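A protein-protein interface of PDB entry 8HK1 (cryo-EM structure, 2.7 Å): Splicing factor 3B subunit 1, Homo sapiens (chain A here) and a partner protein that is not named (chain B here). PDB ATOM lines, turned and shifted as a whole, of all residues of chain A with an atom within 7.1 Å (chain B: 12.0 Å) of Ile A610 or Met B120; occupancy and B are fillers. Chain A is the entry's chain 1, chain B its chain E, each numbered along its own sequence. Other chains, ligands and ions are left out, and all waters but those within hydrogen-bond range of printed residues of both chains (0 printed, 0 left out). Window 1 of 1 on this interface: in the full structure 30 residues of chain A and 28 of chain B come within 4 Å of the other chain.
The backbone carbonyl oxygen of Ala A607 sits at hydrogen-bond distance from the side-chain hydroxyl of Ser A611, 2.5 Å away.
Of the 20 printed residues of chain A, 5 touch a printed residue of chain B. Printed residues of chain A that touch a printed residue of chain B: Ile A610, Ser A611, Arg A614, Phe A647 and Ala A650. Hydrophobic or aromatic side chains of chain A within 4 Å of the printed part of chain B: Ile A610 and Phe A647. Hydrophobic or aromatic side chains of chain B within 4 Å of the printed part of chain A: Leu B116, Phe B119, Met B120, Val B123 and Ala B127.
CG2 of Ile A610 touches CE of Met B120, at 3.8 Å. Val B123 touches Ser A611 (CG1 to OG, 3.6 Å). Ser A611 touches Ala B127. Arg A614 touches Met B120. CE1 of Phe B119 touches CD1 of Phe A647, 3.8 Å away. Ala A650 touches Leu B116 (O to CB, 3.7 Å).
Of chain B, only Met B120 (3.8 Å) comes within 4 Å of Ile A610. Of the printed residues of chain A, Met B120 touches Ile A610 (3.8 Å) and Arg A614 (3.2 Å). No residue of chain B comes within 4 Å of Gly A605. No residue of chain B comes within 4 Å of Leu A606. No residue of chain B comes within 4 Å of Ala A607. Met A609 touches none of the printed residues of chain B. Of chain B, only Val B123 (3.6 Å) and Ala B127 (3.6 Å) come within 4 Å of Ser A611. No residue of chain B comes within 4 Å of Thr A612. No residue of chain B comes within 4 Å of Met A613. Arg A614 touches one residue of chain B. No residue of chain B comes within 4 Å of Leu A644. No residue of chain B comes within 4 Å of Pro A646. Printed residues of chain A within 4 Å of Val B123: Ser A611 (3.6 Å). Of the printed residues of chain A, Phe B119 touches Phe A647. Asp B125 touches none of the printed residues of chain A.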
ATOM      1  N   GLY A 605       4.291  29.655 -21.960  1.00  0.00           N
ATOM      2  CA  GLY A 605       3.130  30.276 -22.552  1.00  0.00           C
ATOM      3  C   GLY A 605       2.268  30.961 -21.503  1.00  0.00           C
ATOM      4  O   GLY A 605       2.520  30.873 -20.297  1.00  0.00           O
ATOM      5  N   LEU A 606       1.237  31.651 -21.987  1.00  0.00           N
ATOM      6  CA  LEU A 606       0.307  32.328 -21.087  1.00  0.00           C
ATOM      7  C   LEU A 606      -0.528  31.325 -20.302  1.00  0.00           C
ATOM      8  O   LEU A 606      -0.765  31.508 -19.100  1.00  0.00           O
ATOM      9  CB  LEU A 606      -0.587  33.273 -21.889  1.00  0.00           C
ATOM     10  CG  LEU A 606      -1.641  34.085 -21.133  1.00  0.00           C
ATOM     11  CD1 LEU A 606      -1.539  35.546 -21.508  1.00  0.00           C
ATOM     12  CD2 LEU A 606      -3.029  33.555 -21.446  1.00  0.00           C
ATOM     13  N   ALA A 607      -0.983  30.260 -20.966  1.00  0.00           N
ATOM     14  CA  ALA A 607      -1.826  29.273 -20.301  1.00  0.00           C
ATOM     15  C   ALA A 607      -1.083  28.583 -19.164  1.00  0.00           C
ATOM     16  O   ALA A 607      -1.662  28.329 -18.103  1.00  0.00           O
ATOM     17  CB  ALA A 607      -2.328  28.245 -21.315  1.00  0.00           C
ATOM     18  N   THR A 608       0.203  28.287 -19.360  1.00  0.00           N
ATOM     19  CA  THR A 608       0.983  27.640 -18.310  1.00  0.00           C
ATOM     20  C   THR A 608       1.130  28.548 -17.094  1.00  0.00           C
ATOM     21  O   THR A 608       0.914  28.117 -15.953  1.00  0.00           O
ATOM     22  CB  THR A 608       2.357  27.240 -18.850  1.00  0.00           C
ATOM     23  OG1 THR A 608       2.201  26.222 -19.845  1.00  0.00           O
ATOM     24  CG2 THR A 608       3.245  26.716 -17.731  1.00  0.00           C
ATOM     25  N   MET A 609       1.500  29.811 -17.323  1.00  0.00           N
ATOM     26  CA  MET A 609       1.638  30.756 -16.219  1.00  0.00           C
ATOM     27  C   MET A 609       0.324  30.906 -15.466  1.00  0.00           C
ATOM     28  O   MET A 609       0.300  30.899 -14.230  1.00  0.00           O
ATOM     29  CB  MET A 609       2.118  32.111 -16.743  1.00  0.00           C
ATOM     30  CG  MET A 609       3.442  32.065 -17.487  1.00  0.00           C
ATOM     31  SD  MET A 609       4.796  31.434 -16.484  1.00  0.00           S
ATOM     32  CE  MET A 609       5.189  32.872 -15.496  1.00  0.00           C
ATOM     33  N   ILE A 610      -0.785  31.025 -16.199  1.00  0.00           N
ATOM     34  CA  ILE A 610      -2.082  31.177 -15.548  1.00  0.00           C
ATOM     35  C   ILE A 610      -2.432  29.929 -14.751  1.00  0.00           C
ATOM     36  O   ILE A 610      -2.948  30.016 -13.631  1.00  0.00           O
ATOM     37  CB  ILE A 610      -3.166  31.512 -16.590  1.00  0.00           C
ATOM     38  CG1 ILE A 610      -3.027  32.963 -17.052  1.00  0.00           C
ATOM     39  CG2 ILE A 610      -4.558  31.269 -16.024  1.00  0.00           C
ATOM     40  CD1 ILE A 610      -4.097  33.394 -18.017  1.00  0.00           C
ATOM     41  N   SER A 611      -2.127  28.747 -15.294  1.00  0.00           N
ATOM     42  CA  SER A 611      -2.515  27.508 -14.627  1.00  0.00           C
ATOM     43  C   SER A 611      -1.697  27.271 -13.367  1.00  0.00           C
ATOM     44  O   SER A 611      -2.192  26.671 -12.405  1.00  0.00           O
ATOM     45  CB  SER A 611      -2.373  26.331 -15.591  1.00  0.00           C
ATOM     46  OG  SER A 611      -3.000  26.608 -16.831  1.00  0.00           O
ATOM     47  N   THR A 612      -0.442  27.725 -13.346  1.00  0.00           N
ATOM     48  CA  THR A 612       0.357  27.560 -12.133  1.00  0.00           C
ATOM     49  C   THR A 612       0.075  28.669 -11.121  1.00  0.00           C
ATOM     50  O   THR A 612       0.228  28.465  -9.910  1.00  0.00           O
ATOM     51  CB  THR A 612       1.852  27.498 -12.461  1.00  0.00           C
ATOM     52  OG1 THR A 612       2.351  28.817 -12.720  1.00  0.00           O
ATOM     53  CG2 THR A 612       2.120  26.580 -13.641  1.00  0.00           C
ATOM     54  N   MET A 613      -0.336  29.848 -11.587  1.00  0.00           N
ATOM     55  CA  MET A 613      -0.556  30.973 -10.686  1.00  0.00           C
ATOM     56  C   MET A 613      -1.985  31.073 -10.165  1.00  0.00           C
ATOM     57  O   MET A 613      -2.218  31.805  -9.198  1.00  0.00           O
ATOM     58  CB  MET A 613      -0.184  32.284 -11.388  1.00  0.00           C
ATOM     59  CG  MET A 613       1.306  32.542 -11.488  1.00  0.00           C
ATOM     60  SD  MET A 613       1.670  34.005 -12.473  1.00  0.00           S
ATOM     61  CE  MET A 613       3.436  34.145 -12.232  1.00  0.00           C
ATOM     62  N   ARG A 614      -2.940  30.366 -10.767  1.00  0.00           N
ATOM     63  CA  ARG A 614      -4.339  30.462 -10.367  1.00  0.00           C
ATOM     64  C   ARG A 614      -4.647  29.876  -8.988  1.00  0.00           C
ATOM     65  O   ARG A 614      -5.498  30.429  -8.280  1.00  0.00           O
ATOM     66  CB  ARG A 614      -5.230  29.791 -11.416  1.00  0.00           C
ATOM     67  CG  ARG A 614      -6.697  30.180 -11.323  1.00  0.00           C
ATOM     68  CD  ARG A 614      -7.526  29.091 -10.665  1.00  0.00           C
ATOM     69  NE  ARG A 614      -8.828  29.583 -10.227  1.00  0.00           N
ATOM     70  CZ  ARG A 614      -9.096  29.988  -8.990  1.00  0.00           C
ATOM     71  NH1 ARG A 614      -8.150  29.961  -8.063  1.00  0.00           N
ATOM     72  NH2 ARG A 614     -10.310  30.421  -8.679  1.00  0.00           N
ATOM     73  N   PRO A 615      -4.025  28.766  -8.564  1.00  0.00           N
ATOM     74  CA  PRO A 615      -4.362  28.241  -7.225  1.00  0.00           C
ATOM     75  C   PRO A 615      -4.029  29.195  -6.092  1.00  0.00           C
ATOM     76  O   PRO A 615      -4.727  29.198  -5.072  1.00  0.00           O
ATOM     77  CB  PRO A 615      -3.547  26.940  -7.135  1.00  0.00           C
ATOM     78  CG  PRO A 615      -2.551  27.010  -8.237  1.00  0.00           C
ATOM     79  CD  PRO A 615      -3.198  27.805  -9.314  1.00  0.00           C
ATOM     80  N   ILE A 617      -4.348  32.384  -6.203  1.00  0.00           N
ATOM     81  CA  ILE A 617      -5.195  33.571  -6.261  1.00  0.00           C
ATOM     82  C   ILE A 617      -6.111  33.627  -5.045  1.00  0.00           C
ATOM     83  O   ILE A 617      -6.336  34.697  -4.465  1.00  0.00           O
ATOM     84  CB  ILE A 617      -5.992  33.586  -7.580  1.00  0.00           C
ATOM     85  CG1 ILE A 617      -5.187  34.254  -8.695  1.00  0.00           C
ATOM     86  CG2 ILE A 617      -7.335  34.281  -7.400  1.00  0.00           C
ATOM     87  CD1 ILE A 617      -5.156  35.757  -8.616  1.00  0.00           C
ATOM     88  N   PHE A 632       1.689  38.582 -11.714  1.00  0.00           N
ATOM     89  CA  PHE A 632       0.718  38.731 -12.794  1.00  0.00           C
ATOM     90  C   PHE A 632       0.915  40.051 -13.531  1.00  0.00           C
ATOM     91  O   PHE A 632       0.773  40.111 -14.757  1.00  0.00           O
ATOM     92  CB  PHE A 632      -0.703  38.623 -12.247  1.00  0.00           C
ATOM     93  CG  PHE A 632      -1.285  37.246 -12.349  1.00  0.00           C
ATOM     94  CD1 PHE A 632      -1.493  36.662 -13.586  1.00  0.00           C
ATOM     95  CD2 PHE A 632      -1.620  36.533 -11.212  1.00  0.00           C
ATOM     96  CE1 PHE A 632      -2.027  35.397 -13.686  1.00  0.00           C
ATOM     97  CE2 PHE A 632      -2.154  35.265 -11.308  1.00  0.00           C
ATOM     98  CZ  PHE A 632      -2.359  34.696 -12.549  1.00  0.00           C
ATOM     99  N   VAL A 635       3.872  39.533 -15.794  1.00  0.00           N
ATOM    100  CA  VAL A 635       3.485  38.727 -16.949  1.00  0.00           C
ATOM    101  C   VAL A 635       2.673  39.553 -17.938  1.00  0.00           C
ATOM    102  O   VAL A 635       2.823  39.400 -19.157  1.00  0.00           O
ATOM    103  CB  VAL A 635       2.712  37.474 -16.492  1.00  0.00           C
ATOM    104  CG1 VAL A 635       2.068  36.769 -17.675  1.00  0.00           C
ATOM    105  CG2 VAL A 635       3.640  36.529 -15.757  1.00  0.00           C
ATOM    106  N   SER A 643      -3.633  40.226 -23.886  1.00  0.00           N
ATOM    107  CA  SER A 643      -3.528  38.781 -23.707  1.00  0.00           C
ATOM    108  C   SER A 643      -4.008  38.352 -22.325  1.00  0.00           C
ATOM    109  O   SER A 643      -4.434  37.205 -22.148  1.00  0.00           O
ATOM    110  CB  SER A 643      -2.087  38.327 -23.933  1.00  0.00           C
ATOM    111  OG  SER A 643      -1.254  38.719 -22.857  1.00  0.00           O
ATOM    112  N   LEU A 644      -3.947  39.249 -21.342  1.00  0.00           N
ATOM    113  CA  LEU A 644      -4.411  38.961 -19.994  1.00  0.00           C
ATOM    114  C   LEU A 644      -5.787  39.545 -19.697  1.00  0.00           C
ATOM    115  O   LEU A 644      -6.377  39.202 -18.667  1.00  0.00           O
ATOM    116  CB  LEU A 644      -3.400  39.490 -18.964  1.00  0.00           C
ATOM    117  CG  LEU A 644      -3.414  38.835 -17.581  1.00  0.00           C
ATOM    118  CD1 LEU A 644      -3.030  37.371 -17.680  1.00  0.00           C
ATOM    119  CD2 LEU A 644      -2.491  39.566 -16.619  1.00  0.00           C
ATOM    120  N   PRO A 646      -8.857  38.928 -20.815  1.00  0.00           N
ATOM    121  CA  PRO A 646      -9.952  37.991 -20.503  1.00  0.00           C
ATOM    122  C   PRO A 646      -9.851  37.363 -19.121  1.00  0.00           C
ATOM    123  O   PRO A 646     -10.864  37.269 -18.415  1.00  0.00           O
ATOM    124  CB  PRO A 646      -9.842  36.933 -21.614  1.00  0.00           C
ATOM    125  CG  PRO A 646      -8.514  37.160 -22.260  1.00  0.00           C
ATOM    126  CD  PRO A 646      -8.232  38.607 -22.109  1.00  0.00           C
ATOM    127  N   PHE A 647      -8.655  36.932 -18.712  1.00  0.00           N
ATOM    128  CA  PHE A 647      -8.495  36.361 -17.378  1.00  0.00           C
ATOM    129  C   PHE A 647      -8.839  37.384 -16.304  1.00  0.00           C
ATOM    130  O   PHE A 647      -9.454  37.049 -15.285  1.00  0.00           O
ATOM    131  CB  PHE A 647      -7.068  35.848 -17.188  1.00  0.00           C
ATOM    132  CG  PHE A 647      -6.775  35.398 -15.784  1.00  0.00           C
ATOM    133  CD1 PHE A 647      -7.370  34.260 -15.269  1.00  0.00           C
ATOM    134  CD2 PHE A 647      -5.909  36.116 -14.977  1.00  0.00           C
ATOM    135  CE1 PHE A 647      -7.104  33.845 -13.978  1.00  0.00           C
ATOM    136  CE2 PHE A 647      -5.640  35.707 -13.687  1.00  0.00           C
ATOM    137  CZ  PHE A 647      -6.241  34.569 -13.188  1.00  0.00           C
ATOM    138  N   LEU A 648      -8.443  38.641 -16.513  1.00  0.00           N
ATOM    139  CA  LEU A 648      -8.799  39.692 -15.566  1.00  0.00           C
ATOM    140  C   LEU A 648     -10.306  39.883 -15.504  1.00  0.00           C
ATOM    141  O   LEU A 648     -10.900  39.825 -14.423  1.00  0.00           O
ATOM    142  CB  LEU A 648      -8.108  40.999 -15.945  1.00  0.00           C
ATOM    143  CG  LEU A 648      -6.591  41.005 -15.754  1.00  0.00           C
ATOM    144  CD1 LEU A 648      -5.995  42.335 -16.174  1.00  0.00           C
ATOM    145  CD2 LEU A 648      -6.251  40.692 -14.311  1.00  0.00           C
ATOM    146  N   ALA A 650     -12.567  37.894 -16.107  1.00  0.00           N
ATOM    147  CA  ALA A 650     -13.209  36.756 -15.461  1.00  0.00           C
ATOM    148  C   ALA A 650     -12.955  36.719 -13.958  1.00  0.00           C
ATOM    149  O   ALA A 650     -13.861  36.371 -13.195  1.00  0.00           O
ATOM    150  CB  ALA A 650     -12.734  35.451 -16.100  1.00  0.00           C
ATOM    151  N   ASP B 114     -19.045  30.943 -12.014  1.00  0.00           N
ATOM    152  CA  ASP B 114     -19.530  30.112 -13.149  1.00  0.00           C
ATOM    153  C   ASP B 114     -18.698  30.424 -14.398  1.00  0.00           C
ATOM    154  O   ASP B 114     -18.013  29.508 -14.895  1.00  0.00           O
ATOM    155  CB  ASP B 114     -21.024  30.326 -13.405  1.00  0.00           C
ATOM    156  CG  ASP B 114     -21.916  29.649 -12.379  1.00  0.00           C
ATOM    157  OD1 ASP B 114     -21.445  28.692 -11.733  1.00  0.00           O
ATOM    158  OD2 ASP B 114     -23.076  30.082 -12.236  1.00  0.00           O
ATOM    159  N   PRO B 115     -18.721  31.671 -14.920  1.00  0.00           N
ATOM    160  CA  PRO B 115     -17.950  32.022 -16.117  1.00  0.00           C
ATOM    161  C   PRO B 115     -16.450  31.856 -15.842  1.00  0.00           C
ATOM    162  O   PRO B 115     -15.751  31.323 -16.690  1.00  0.00           O
ATOM    163  CB  PRO B 115     -18.293  33.499 -16.353  1.00  0.00           C
ATOM    164  CG  PRO B 115     -18.759  33.995 -15.001  1.00  0.00           C
ATOM    165  CD  PRO B 115     -19.465  32.807 -14.380  1.00  0.00           C
ATOM    166  N   LEU B 116     -16.007  32.277 -14.654  1.00  0.00           N
ATOM    167  CA  LEU B 116     -14.576  32.157 -14.273  1.00  0.00           C
ATOM    168  C   LEU B 116     -14.210  30.670 -14.259  1.00  0.00           C
ATOM    169  O   LEU B 116     -13.162  30.318 -14.827  1.00  0.00           O
ATOM    170  CB  LEU B 116     -14.394  32.772 -12.882  1.00  0.00           C
ATOM    171  CG  LEU B 116     -12.997  32.649 -12.273  1.00  0.00           C
ATOM    172  CD1 LEU B 116     -12.859  33.544 -11.051  1.00  0.00           C
ATOM    173  CD2 LEU B 116     -12.682  31.207 -11.910  1.00  0.00           C
ATOM    174  N   GLU B 117     -15.087  29.833 -13.697  1.00  0.00           N
ATOM    175  CA  GLU B 117     -14.827  28.372 -13.619  1.00  0.00           C
ATOM    176  C   GLU B 117     -14.718  27.806 -15.037  1.00  0.00           C
ATOM    177  O   GLU B 117     -13.772  27.037 -15.290  1.00  0.00           O
ATOM    178  CB  GLU B 117     -15.974  27.685 -12.876  1.00  0.00           C
ATOM    179  CG  GLU B 117     -16.098  28.097 -11.419  1.00  0.00           C
ATOM    180  CD  GLU B 117     -15.392  27.181 -10.435  1.00  0.00           C
ATOM    181  OE1 GLU B 117     -14.988  26.074 -10.844  1.00  0.00           O
ATOM    182  OE2 GLU B 117     -15.252  27.574  -9.259  1.00  0.00           O
ATOM    183  N   ALA B 118     -15.616  28.220 -15.937  1.00  0.00           N
ATOM    184  CA  ALA B 118     -15.603  27.710 -17.327  1.00  0.00           C
ATOM    185  C   ALA B 118     -14.296  28.121 -18.011  1.00  0.00           C
ATOM    186  O   ALA B 118     -13.655  27.256 -18.666  1.00  0.00           O
ATOM    187  CB  ALA B 118     -16.800  28.245 -18.073  1.00  0.00           C
ATOM    188  N   PHE B 119     -13.883  29.376 -17.802  1.00  0.00           N
ATOM    189  CA  PHE B 119     -12.638  29.885 -18.431  1.00  0.00           C
ATOM    190  C   PHE B 119     -11.461  29.060 -17.906  1.00  0.00           C
ATOM    191  O   PHE B 119     -10.632  28.606 -18.718  1.00  0.00           O
ATOM    192  CB  PHE B 119     -12.452  31.369 -18.101  1.00  0.00           C
ATOM    193  CG  PHE B 119     -11.145  31.960 -18.565  1.00  0.00           C
ATOM    194  CD1 PHE B 119     -10.005  31.864 -17.783  1.00  0.00           C
ATOM    195  CD2 PHE B 119     -11.052  32.611 -19.784  1.00  0.00           C
ATOM    196  CE1 PHE B 119      -8.803  32.404 -18.210  1.00  0.00           C
ATOM    197  CE2 PHE B 119      -9.849  33.149 -20.212  1.00  0.00           C
ATOM    198  CZ  PHE B 119      -8.727  33.044 -19.425  1.00  0.00           C
ATOM    199  N   MET B 120     -11.452  28.801 -16.595  1.00  0.00           N
ATOM    200  CA  MET B 120     -10.350  28.031 -15.967  1.00  0.00           C
ATOM    201  C   MET B 120     -10.318  26.622 -16.559  1.00  0.00           C
ATOM    202  O   MET B 120      -9.227  26.176 -16.907  1.00  0.00           O
ATOM    203  CB  MET B 120     -10.538  27.939 -14.448  1.00  0.00           C
ATOM    204  CG  MET B 120      -9.766  28.997 -13.681  1.00  0.00           C
ATOM    205  SD  MET B 120      -7.977  28.880 -13.944  1.00  0.00           S
ATOM    206  CE  MET B 120      -7.859  29.390 -15.658  1.00  0.00           C
ATOM    207  N   ALA B 121     -11.480  25.989 -16.731  1.00  0.00           N
ATOM    208  CA  ALA B 121     -11.519  24.616 -17.288  1.00  0.00           C
ATOM    209  C   ALA B 121     -10.961  24.621 -18.715  1.00  0.00           C
ATOM    210  O   ALA B 121     -10.103  23.758 -19.020  1.00  0.00           O
ATOM    211  CB  ALA B 121     -12.935  24.098 -17.255  1.00  0.00           C
ATOM    212  N   GLU B 122     -11.365  25.600 -19.533  1.00  0.00           N
ATOM    213  CA  GLU B 122     -10.865  25.631 -20.934  1.00  0.00           C
ATOM    214  C   GLU B 122      -9.344  25.818 -20.915  1.00  0.00           C
ATOM    215  O   GLU B 122      -8.634  25.081 -21.651  1.00  0.00           O
ATOM    216  CB  GLU B 122     -11.516  26.779 -21.707  1.00  0.00           C
ATOM    217  CG  GLU B 122     -12.962  26.516 -22.085  1.00  0.00           C
ATOM    218  CD  GLU B 122     -13.548  27.548 -23.033  1.00  0.00           C
ATOM    219  OE1 GLU B 122     -12.841  28.528 -23.341  1.00  0.00           O
ATOM    220  OE2 GLU B 122     -14.704  27.369 -23.463  1.00  0.00           O
ATOM    221  N   VAL B 123      -8.866  26.717 -20.050  1.00  0.00           N
ATOM    222  CA  VAL B 123      -7.408  27.018 -19.968  1.00  0.00           C
ATOM    223  C   VAL B 123      -6.668  25.751 -19.538  1.00  0.00           C
ATOM    224  O   VAL B 123      -5.651  25.435 -20.159  1.00  0.00           O
ATOM    225  CB  VAL B 123      -7.134  28.182 -18.996  1.00  0.00           C
ATOM    226  CG1 VAL B 123      -5.657  28.291 -18.650  1.00  0.00           C
ATOM    227  CG2 VAL B 123      -7.653  29.499 -19.549  1.00  0.00           C
ATOM    228  N   GLU B 124      -7.213  25.024 -18.561  1.00  0.00           N
ATOM    229  CA  GLU B 124      -6.561  23.791 -18.054  1.00  0.00           C
ATOM    230  C   GLU B 124      -6.484  22.776 -19.194  1.00  0.00           C
ATOM    231  O   GLU B 124      -5.396  22.231 -19.404  1.00  0.00           O
ATOM    232  CB  GLU B 124      -7.353  23.216 -16.877  1.00  0.00           C
ATOM    233  CG  GLU B 124      -7.217  24.027 -15.603  1.00  0.00           C
ATOM    234  CD  GLU B 124      -8.179  23.633 -14.496  1.00  0.00           C
ATOM    235  OE1 GLU B 124      -8.758  22.530 -14.582  1.00  0.00           O
ATOM    236  OE2 GLU B 124      -8.355  24.432 -13.555  1.00  0.00           O
ATOM    237  N   ASP B 125      -7.566  22.612 -19.960  1.00  0.00           N
ATOM    238  CA  ASP B 125      -7.523  21.615 -21.062  1.00  0.00           C
ATOM    239  C   ASP B 125      -6.438  22.024 -22.066  1.00  0.00           C
ATOM    240  O   ASP B 125      -5.581  21.168 -22.398  1.00  0.00           O
ATOM    241  CB  ASP B 125      -8.885  21.492 -21.749  1.00  0.00           C
ATOM    242  CG  ASP B 125      -9.924  20.755 -20.919  1.00  0.00           C
ATOM    243  OD1 ASP B 125      -9.542  20.175 -19.885  1.00  0.00           O
ATOM    244  OD2 ASP B 125     -11.108  20.770 -21.315  1.00  0.00           O
ATOM    245  N   GLN B 126      -6.398  23.309 -22.433  1.00  0.00           N
ATOM    246  CA  GLN B 126      -5.403  23.756 -23.444  1.00  0.00           C
ATOM    247  C   GLN B 126      -3.984  23.533 -22.906  1.00  0.00           C
ATOM    248  O   GLN B 126      -3.139  22.985 -23.651  1.00  0.00           O
ATOM    249  CB  GLN B 126      -5.625  25.237 -23.761  1.00  0.00           C
ATOM    250  CG  GLN B 126      -5.801  25.533 -25.243  1.00  0.00           C
ATOM    251  CD  GLN B 126      -4.647  25.043 -26.083  1.00  0.00           C
ATOM    252  OE1 GLN B 126      -3.623  24.598 -25.569  1.00  0.00           O
ATOM    253  NE2 GLN B 126      -4.806  25.123 -27.393  1.00  0.00           N
ATOM    254  N   ALA B 127      -3.761  23.880 -21.637  1.00  0.00           N
ATOM    255  CA  ALA B 127      -2.427  23.763 -21.005  1.00  0.00           C
ATOM    256  C   ALA B 127      -2.009  22.293 -20.958  1.00  0.00           C
ATOM    257  O   ALA B 127      -0.855  22.003 -21.300  1.00  0.00           O
ATOM    258  CB  ALA B 127      -2.467  24.367 -19.622  1.00  0.00           C
ATOM    259  N   ALA B 128      -2.939  21.405 -20.602  1.00  0.00           N
ATOM    260  CA  ALA B 128      -2.629  19.961 -20.517  1.00  0.00           C
ATOM    261  C   ALA B 128      -2.239  19.472 -21.910  1.00  0.00           C
ATOM    262  O   ALA B 128      -1.201  18.804 -22.027  1.00  0.00           O
ATOM    263  CB  ALA B 128      -3.826  19.211 -19.985  1.00  0.00           C
ATOM    264  N   ARG B 129      -2.987  19.887 -22.936  1.00  0.00           N
ATOM    265  CA  ARG B 129      -2.666  19.424 -24.309  1.00  0.00           C
ATOM    266  C   ARG B 129      -1.259  19.906 -24.680  1.00  0.00           C
ATOM    267  O   ARG B 129      -0.453  19.073 -25.142  1.00  0.00           O
ATOM    268  CB  ARG B 129      -3.681  19.994 -25.304  1.00  0.00           C
ATOM    269  CG  ARG B 129      -5.068  19.373 -25.215  1.00  0.00           C
ATOM    270  CD  ARG B 129      -6.134  20.377 -25.610  1.00  0.00           C
ATOM    271  NE  ARG B 129      -5.624  21.385 -26.529  1.00  0.00           N
ATOM    272  CZ  ARG B 129      -5.748  21.335 -27.850  1.00  0.00           C
ATOM    273  NH1 ARG B 129      -6.373  20.318 -28.418  1.00  0.00           N
ATOM    274  NH2 ARG B 129      -5.247  22.301 -28.598  1.00  0.00           N
ATOM    275  N   ASP B 130      -0.949  21.173 -24.390  1.00  0.00           N
ATOM    276  CA  ASP B 130       0.380  21.728 -24.765  1.00  0.00           C
ATOM    277  C   ASP B 130       1.491  20.982 -24.016  1.00  0.00           C
ATOM    278  O   ASP B 130       2.502  20.617 -24.660  1.00  0.00           O
ATOM    279  CB  ASP B 130       0.434  23.236 -24.514  1.00  0.00           C
ATOM    280  CG  ASP B 130       1.086  24.000 -25.653  1.00  0.00           C
ATOM    281  OD1 ASP B 130       1.483  23.347 -26.642  1.00  0.00           O
ATOM    282  OD2 ASP B 130       1.180  25.239 -25.550  1.00  0.00           O
ATOM    283  N   MET B 131       1.281  20.716 -22.724  1.00  0.00           N
ATOM    284  CA  MET B 131       2.302  20.030 -21.891  1.00  0.00           C
ATOM    285  C   MET B 131       2.524  18.626 -22.456  1.00  0.00           C
ATOM    286  O   MET B 131       3.695  18.234 -22.627  1.00  0.00           O
ATOM    287  CB  MET B 131       1.816  19.913 -20.444  1.00  0.00           C
ATOM    288  CG  MET B 131       2.896  19.481 -19.473  1.00  0.00           C
ATOM    289  SD  MET B 131       4.165  20.754 -19.260  1.00  0.00           S
ATOM    290  CE  MET B 131       5.223  19.977 -18.039  1.00  0.00           C
